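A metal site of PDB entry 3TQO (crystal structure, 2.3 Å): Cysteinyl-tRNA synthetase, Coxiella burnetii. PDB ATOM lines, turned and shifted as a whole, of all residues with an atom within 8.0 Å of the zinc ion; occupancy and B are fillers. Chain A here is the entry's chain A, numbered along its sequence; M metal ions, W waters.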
ATOM      1  N   TYR A  29     -20.255 -30.549 -26.835  1.00  0.00           N
ATOM      2  CA  TYR A  29     -21.045 -29.667 -25.991  1.00  0.00           C
ATOM      3  C   TYR A  29     -20.174 -29.147 -24.857  1.00  0.00           C
ATOM      4  O   TYR A  29     -19.494 -29.919 -24.174  1.00  0.00           O
ATOM      5  CB  TYR A  29     -22.258 -30.397 -25.424  1.00  0.00           C
ATOM      6  CG  TYR A  29     -23.215 -29.524 -24.645  1.00  0.00           C
ATOM      7  CD1 TYR A  29     -24.210 -28.804 -25.289  1.00  0.00           C
ATOM      8  CD2 TYR A  29     -23.133 -29.435 -23.261  1.00  0.00           C
ATOM      9  CE1 TYR A  29     -25.098 -28.011 -24.577  1.00  0.00           C
ATOM     10  CE2 TYR A  29     -24.009 -28.646 -22.543  1.00  0.00           C
ATOM     11  CZ  TYR A  29     -24.993 -27.940 -23.200  1.00  0.00           C
ATOM     12  OH  TYR A  29     -25.869 -27.151 -22.481  1.00  0.00           O
ATOM     13  N   VAL A  30     -20.189 -27.832 -24.647  1.00  0.00           N
ATOM     14  CA  VAL A  30     -19.456 -27.239 -23.539  1.00  0.00           C
ATOM     15  C   VAL A  30     -20.404 -26.381 -22.705  1.00  0.00           C
ATOM     16  O   VAL A  30     -21.173 -25.584 -23.251  1.00  0.00           O
ATOM     17  CB  VAL A  30     -18.286 -26.369 -24.038  1.00  0.00           C
ATOM     18  CG1 VAL A  30     -17.586 -25.697 -22.871  1.00  0.00           C
ATOM     19  CG2 VAL A  30     -17.307 -27.210 -24.843  1.00  0.00           C
ATOM     20  N   CYS A  31     -20.376 -26.555 -21.382  1.00  0.00           N
ATOM     21  CA  CYS A  31     -21.213 -25.748 -20.506  1.00  0.00           C
ATOM     22  C   CYS A  31     -20.803 -24.275 -20.581  1.00  0.00           C
ATOM     23  O   CYS A  31     -19.617 -23.942 -20.541  1.00  0.00           O
ATOM     24  CB  CYS A  31     -21.170 -26.253 -19.063  1.00  0.00           C
ATOM     25  SG  CYS A  31     -21.970 -27.877 -18.827  1.00  0.00           S
ATOM     26  N   GLY A  32     -21.799 -23.395 -20.690  1.00  0.00           N
ATOM     27  CA  GLY A  32     -21.540 -21.974 -20.854  1.00  0.00           C
ATOM     28  C   GLY A  32     -21.847 -21.116 -19.654  1.00  0.00           C
ATOM     29  O   GLY A  32     -21.815 -21.570 -18.510  1.00  0.00           O
ATOM     30  N   MET A  33     -22.162 -19.853 -19.925  1.00  0.00           N
ATOM     31  CA  MET A  33     -22.315 -18.829 -18.897  1.00  0.00           C
ATOM     32  C   MET A  33     -23.711 -18.752 -18.273  1.00  0.00           C
ATOM     33  O   MET A  33     -24.718 -18.912 -18.958  1.00  0.00           O
ATOM     34  CB  MET A  33     -21.966 -17.467 -19.505  1.00  0.00           C
ATOM     35  CG  MET A  33     -21.846 -16.347 -18.491  1.00  0.00           C
ATOM     36  SD  MET A  33     -20.319 -16.432 -17.548  1.00  0.00           S
ATOM     37  CE  MET A  33     -20.660 -15.230 -16.251  1.00  0.00           C
ATOM     38  N   THR A  34     -23.757 -18.504 -16.967  1.00  0.00           N
ATOM     39  CA  THR A  34     -24.982 -18.097 -16.294  1.00  0.00           C
ATOM     40  C   THR A  34     -25.022 -16.576 -16.332  1.00  0.00           C
ATOM     41  O   THR A  34     -24.222 -15.917 -15.668  1.00  0.00           O
ATOM     42  CB  THR A  34     -25.013 -18.559 -14.829  1.00  0.00           C
ATOM     43  OG1 THR A  34     -24.865 -19.982 -14.784  1.00  0.00           O
ATOM     44  CG2 THR A  34     -26.320 -18.150 -14.157  1.00  0.00           C
ATOM     45  N   ASN A  69     -24.077 -23.602 -24.440  1.00  0.00           N
ATOM     46  CA  ASN A  69     -25.354 -23.063 -23.975  1.00  0.00           C
ATOM     47  C   ASN A  69     -25.236 -21.765 -23.190  1.00  0.00           C
ATOM     48  O   ASN A  69     -24.176 -21.431 -22.652  1.00  0.00           O
ATOM     49  CB  ASN A  69     -26.066 -24.103 -23.122  1.00  0.00           C
ATOM     50  CG  ASN A  69     -25.425 -24.273 -21.755  1.00  0.00           C
ATOM     51  OD1 ASN A  69     -24.316 -24.787 -21.645  1.00  0.00           O
ATOM     52  ND2 ASN A  69     -26.130 -23.839 -20.708  1.00  0.00           N
ATOM     53  N   THR A  71     -27.074 -20.247 -19.891  1.00  0.00           N
ATOM     54  CA  THR A  71     -27.999 -20.515 -18.796  1.00  0.00           C
ATOM     55  C   THR A  71     -28.739 -19.242 -18.433  1.00  0.00           C
ATOM     56  O   THR A  71     -28.241 -18.431 -17.653  1.00  0.00           O
ATOM     57  CB  THR A  71     -27.280 -21.061 -17.554  1.00  0.00           C
ATOM     58  OG1 THR A  71     -26.438 -22.157 -17.919  1.00  0.00           O
ATOM     59  CG2 THR A  71     -28.300 -21.518 -16.508  1.00  0.00           C
ATOM     60  N   TRP A 208     -31.046 -26.768 -12.758  1.00  0.00           N
ATOM     61  CA  TRP A 208     -29.900 -26.392 -13.585  1.00  0.00           C
ATOM     62  C   TRP A 208     -29.454 -27.526 -14.509  1.00  0.00           C
ATOM     63  O   TRP A 208     -29.279 -27.328 -15.702  1.00  0.00           O
ATOM     64  CB  TRP A 208     -28.739 -25.958 -12.677  1.00  0.00           C
ATOM     65  CG  TRP A 208     -27.464 -25.644 -13.405  1.00  0.00           C
ATOM     66  CD1 TRP A 208     -27.338 -25.214 -14.693  1.00  0.00           C
ATOM     67  CD2 TRP A 208     -26.143 -25.749 -12.870  1.00  0.00           C
ATOM     68  NE1 TRP A 208     -26.010 -25.033 -14.995  1.00  0.00           N
ATOM     69  CE2 TRP A 208     -25.254 -25.353 -13.902  1.00  0.00           C
ATOM     70  CE3 TRP A 208     -25.618 -26.125 -11.634  1.00  0.00           C
ATOM     71  CZ2 TRP A 208     -23.870 -25.332 -13.720  1.00  0.00           C
ATOM     72  CZ3 TRP A 208     -24.243 -26.109 -11.454  1.00  0.00           C
ATOM     73  CH2 TRP A 208     -23.387 -25.710 -12.500  1.00  0.00           C
ATOM     74  N   HIS A 209     -29.276 -28.717 -13.933  1.00  0.00           N
ATOM     75  CA  HIS A 209     -28.689 -29.844 -14.665  1.00  0.00           C
ATOM     76  C   HIS A 209     -29.556 -30.367 -15.808  1.00  0.00           C
ATOM     77  O   HIS A 209     -29.045 -30.712 -16.876  1.00  0.00           O
ATOM     78  CB  HIS A 209     -28.369 -30.978 -13.697  1.00  0.00           C
ATOM     79  CG  HIS A 209     -28.024 -30.499 -12.317  1.00  0.00           C
ATOM     80  ND1 HIS A 209     -26.909 -29.738 -12.043  1.00  0.00           N
ATOM     81  CD2 HIS A 209     -28.663 -30.668 -11.131  1.00  0.00           C
ATOM     82  CE1 HIS A 209     -26.871 -29.466 -10.757  1.00  0.00           C
ATOM     83  NE2 HIS A 209     -27.921 -30.012 -10.181  1.00  0.00           N
ATOM     84  N   ILE A 210     -30.860 -30.435 -15.585  1.00  0.00           N
ATOM     85  CA  ILE A 210     -31.775 -30.992 -16.574  1.00  0.00           C
ATOM     86  C   ILE A 210     -31.784 -30.111 -17.824  1.00  0.00           C
ATOM     87  O   ILE A 210     -32.092 -30.576 -18.919  1.00  0.00           O
ATOM     88  CB  ILE A 210     -33.207 -31.128 -16.000  1.00  0.00           C
ATOM     89  CG1 ILE A 210     -34.021 -32.126 -16.829  1.00  0.00           C
ATOM     90  CG2 ILE A 210     -33.893 -29.769 -15.898  1.00  0.00           C
ATOM     91  CD1 ILE A 210     -33.653 -33.574 -16.558  1.00  0.00           C
ATOM     92  N   GLU A 211     -31.428 -28.850 -17.647  1.00  0.00           N
ATOM     93  CA  GLU A 211     -31.315 -27.922 -18.772  1.00  0.00           C
ATOM     94  C   GLU A 211     -30.258 -28.380 -19.781  1.00  0.00           C
ATOM     95  O   GLU A 211     -30.516 -28.428 -20.977  1.00  0.00           O
ATOM     96  CB  GLU A 211     -30.986 -26.515 -18.285  1.00  0.00           C
ATOM     97  CG  GLU A 211     -32.064 -25.883 -17.407  1.00  0.00           C
ATOM     98  CD  GLU A 211     -31.657 -24.540 -16.852  1.00  0.00           C
ATOM     99  OE1 GLU A 211     -32.480 -23.896 -16.173  1.00  0.00           O
ATOM    100  OE2 GLU A 211     -30.495 -24.122 -17.082  1.00  0.00           O
ATOM    101  N   CYS A 212     -29.069 -28.719 -19.281  1.00  0.00           N
ATOM    102  CA  CYS A 212     -27.976 -29.124 -20.157  1.00  0.00           C
ATOM    103  C   CYS A 212     -28.165 -30.553 -20.705  1.00  0.00           C
ATOM    104  O   CYS A 212     -27.765 -30.837 -21.841  1.00  0.00           O
ATOM    105  CB  CYS A 212     -26.627 -28.962 -19.448  1.00  0.00           C
ATOM    106  SG  CYS A 212     -26.163 -27.216 -19.158  1.00  0.00           S
ATOM    107  N   SER A 213     -28.766 -31.433 -19.912  1.00  0.00           N
ATOM    108  CA  SER A 213     -29.101 -32.767 -20.395  1.00  0.00           C
ATOM    109  C   SER A 213     -30.032 -32.697 -21.604  1.00  0.00           C
ATOM    110  O   SER A 213     -29.850 -33.405 -22.590  1.00  0.00           O
ATOM    111  CB  SER A 213     -29.764 -33.606 -19.300  1.00  0.00           C
ATOM    112  OG  SER A 213     -28.798 -34.166 -18.431  1.00  0.00           O
ATOM    113  N   MET A 215     -30.829 -29.873 -23.561  1.00  0.00           N
ATOM    114  CA  MET A 215     -30.301 -29.077 -24.673  1.00  0.00           C
ATOM    115  C   MET A 215     -29.250 -29.839 -25.478  1.00  0.00           C
ATOM    116  O   MET A 215     -29.300 -29.853 -26.706  1.00  0.00           O
ATOM    117  CB  MET A 215     -29.728 -27.742 -24.173  1.00  0.00           C
ATOM    118  CG  MET A 215     -30.796 -26.720 -23.746  1.00  0.00           C
ATOM    119  SD  MET A 215     -30.146 -25.071 -23.378  1.00  0.00           S
ATOM    120  CE  MET A 215     -29.148 -25.402 -21.918  1.00  0.00           C
ATOM    121  N   HIS A 227     -18.026 -33.830 -24.073  1.00  0.00           N
ATOM    122  CA  HIS A 227     -18.698 -32.879 -23.195  1.00  0.00           C
ATOM    123  C   HIS A 227     -17.633 -32.203 -22.349  1.00  0.00           C
ATOM    124  O   HIS A 227     -16.778 -32.873 -21.771  1.00  0.00           O
ATOM    125  CB  HIS A 227     -19.738 -33.598 -22.322  1.00  0.00           C
ATOM    126  CG  HIS A 227     -20.735 -32.678 -21.692  1.00  0.00           C
ATOM    127  ND1 HIS A 227     -20.401 -31.445 -21.171  1.00  0.00           N
ATOM    128  CD2 HIS A 227     -22.075 -32.816 -21.502  1.00  0.00           C
ATOM    129  CE1 HIS A 227     -21.485 -30.863 -20.689  1.00  0.00           C
ATOM    130  NE2 HIS A 227     -22.511 -31.671 -20.875  1.00  0.00           N
ATOM    131  N   GLY A 228     -17.676 -30.885 -22.289  1.00  0.00           N
ATOM    132  CA  GLY A 228     -16.644 -30.133 -21.588  1.00  0.00           C
ATOM    133  C   GLY A 228     -17.182 -29.133 -20.593  1.00  0.00           C
ATOM    134  O   GLY A 228     -18.398 -28.907 -20.501  1.00  0.00           O
ATOM    135  N   GLY A 229     -16.269 -28.525 -19.841  1.00  0.00           N
ATOM    136  CA  GLY A 229     -16.610 -27.521 -18.859  1.00  0.00           C
ATOM    137  C   GLY A 229     -15.473 -27.333 -17.869  1.00  0.00           C
ATOM    138  O   GLY A 229     -14.438 -27.997 -17.951  1.00  0.00           O
ATOM    139  N   LEU A 233     -17.524 -28.125 -12.533  1.00  0.00           N
ATOM    140  CA  LEU A 233     -18.815 -28.587 -13.014  1.00  0.00           C
ATOM    141  C   LEU A 233     -18.899 -30.114 -12.979  1.00  0.00           C
ATOM    142  O   LEU A 233     -19.981 -30.678 -13.142  1.00  0.00           O
ATOM    143  CB  LEU A 233     -19.087 -28.078 -14.426  1.00  0.00           C
ATOM    144  CG  LEU A 233     -19.087 -26.563 -14.639  1.00  0.00           C
ATOM    145  CD1 LEU A 233     -19.558 -26.222 -16.047  1.00  0.00           C
ATOM    146  CD2 LEU A 233     -19.937 -25.862 -13.592  1.00  0.00           C
ATOM    147  N   HIS A 237     -22.718 -31.129 -11.131  1.00  0.00           N
ATOM    148  CA  HIS A 237     -23.373 -30.783 -12.387  1.00  0.00           C
ATOM    149  C   HIS A 237     -23.307 -31.855 -13.480  1.00  0.00           C
ATOM    150  O   HIS A 237     -24.343 -32.352 -13.935  1.00  0.00           O
ATOM    151  CB  HIS A 237     -22.833 -29.460 -12.925  1.00  0.00           C
ATOM    152  CG  HIS A 237     -23.603 -28.916 -14.086  1.00  0.00           C
ATOM    153  ND1 HIS A 237     -24.986 -28.836 -14.087  1.00  0.00           N
ATOM    154  CD2 HIS A 237     -23.199 -28.436 -15.278  1.00  0.00           C
ATOM    155  CE1 HIS A 237     -25.385 -28.321 -15.233  1.00  0.00           C
ATOM    156  NE2 HIS A 237     -24.321 -28.064 -15.969  1.00  0.00           N
ATOM    157  N   HIS A 238     -22.098 -32.197 -13.909  1.00  0.00           N
ATOM    158  CA  HIS A 238     -21.922 -33.188 -14.963  1.00  0.00           C
ATOM    159  C   HIS A 238     -22.370 -34.570 -14.491  1.00  0.00           C
ATOM    160  O   HIS A 238     -22.945 -35.332 -15.253  1.00  0.00           O
ATOM    161  CB  HIS A 238     -20.471 -33.233 -15.438  1.00  0.00           C
ATOM    162  CG  HIS A 238     -20.046 -32.005 -16.171  1.00  0.00           C
ATOM    163  ND1 HIS A 238     -20.936 -31.095 -16.706  1.00  0.00           N
ATOM    164  CD2 HIS A 238     -18.808 -31.532 -16.471  1.00  0.00           C
ATOM    165  CE1 HIS A 238     -20.268 -30.119 -17.290  1.00  0.00           C
ATOM    166  NE2 HIS A 238     -18.974 -30.361 -17.161  1.00  0.00           N
ATOM    167  N   GLU A 241     -26.033 -34.645 -14.911  1.00  0.00           N
ATOM    168  CA  GLU A 241     -26.380 -34.720 -16.329  1.00  0.00           C
ATOM    169  C   GLU A 241     -26.364 -36.165 -16.821  1.00  0.00           C
ATOM    170  O   GLU A 241     -27.281 -36.597 -17.515  1.00  0.00           O
ATOM    171  CB  GLU A 241     -25.437 -33.890 -17.192  1.00  0.00           C
ATOM    172  CG  GLU A 241     -25.772 -32.411 -17.255  1.00  0.00           C
ATOM    173  CD  GLU A 241     -24.883 -31.653 -18.227  1.00  0.00           C
ATOM    174  OE1 GLU A 241     -24.903 -31.986 -19.438  1.00  0.00           O
ATOM    175  OE2 GLU A 241     -24.164 -30.742 -17.771  1.00  0.00           O
ATOM    176  N   TRP A 257     -15.254 -37.073 -21.573  1.00  0.00           N
ATOM    177  CA  TRP A 257     -15.411 -35.881 -20.746  1.00  0.00           C
ATOM    178  C   TRP A 257     -14.098 -35.118 -20.597  1.00  0.00           C
ATOM    179  O   TRP A 257     -13.083 -35.678 -20.189  1.00  0.00           O
ATOM    180  CB  TRP A 257     -15.950 -36.267 -19.369  1.00  0.00           C
ATOM    181  CG  TRP A 257     -17.395 -36.668 -19.376  1.00  0.00           C
ATOM    182  CD1 TRP A 257     -17.903 -37.924 -19.559  1.00  0.00           C
ATOM    183  CD2 TRP A 257     -18.528 -35.802 -19.181  1.00  0.00           C
ATOM    184  NE1 TRP A 257     -19.272 -37.892 -19.503  1.00  0.00           N
ATOM    185  CE2 TRP A 257     -19.682 -36.601 -19.274  1.00  0.00           C
ATOM    186  CE3 TRP A 257     -18.668 -34.432 -18.952  1.00  0.00           C
ATOM    187  CZ2 TRP A 257     -20.965 -36.080 -19.126  1.00  0.00           C
ATOM    188  CZ3 TRP A 257     -19.951 -33.906 -18.817  1.00  0.00           C
ATOM    189  CH2 TRP A 257     -21.079 -34.737 -18.899  1.00  0.00           C
HETATM  190 ZN    ZN M   1     -24.078 -27.201 -18.000  1.00  0.00          ZN
HETATM  191  O   HOH W   1     -24.151 -24.804 -17.705  1.00  0.00           O
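O of Gly 228 is in hydrogen-bond range of N of Cys 31. The side-chain hydroxyl (OH) of Tyr 29 sits close to the side-chain sulfur (SG) of Cys 212 (3.3 Å). The side-chain carboxylate (OE1) of Glu 241 is in hydrogen-bond range of a ring nitrogen (NE2) of His 227. OE2 of Glu 241 lies within hydrogen-bond range of ND1 of His 238. OE2 of Glu 241 lies close to SG of Cys 31 (3.8 Å). A ring nitrogen (ND1) of His 209 lies within hydrogen-bond range of a ring nitrogen (ND1) of His 237, 2.9 Å away. The side-chain carboxylate (OE2) of Glu 241 sits close to a ring nitrogen (NE2) of His 237 (3.2 Å). SG of Cys 212 sits close to ND2 of Asn 69.
Merely in contact with the zinc ion: Glu 241 (3.5 Å). Within 4 Å of the zinc ion: Cys 31, Cys 212, His 237 and Glu 241. The nearest printed residue that does not touch the zinc ion is Trp 208 (4.2 Å).
The zinc ion is bound by NE2 of His 237 (2.2 Å), SG of Cys 31 (2.4 Å), SG of Cys 212 (2.4 Å) and water W1 (2.4 Å).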
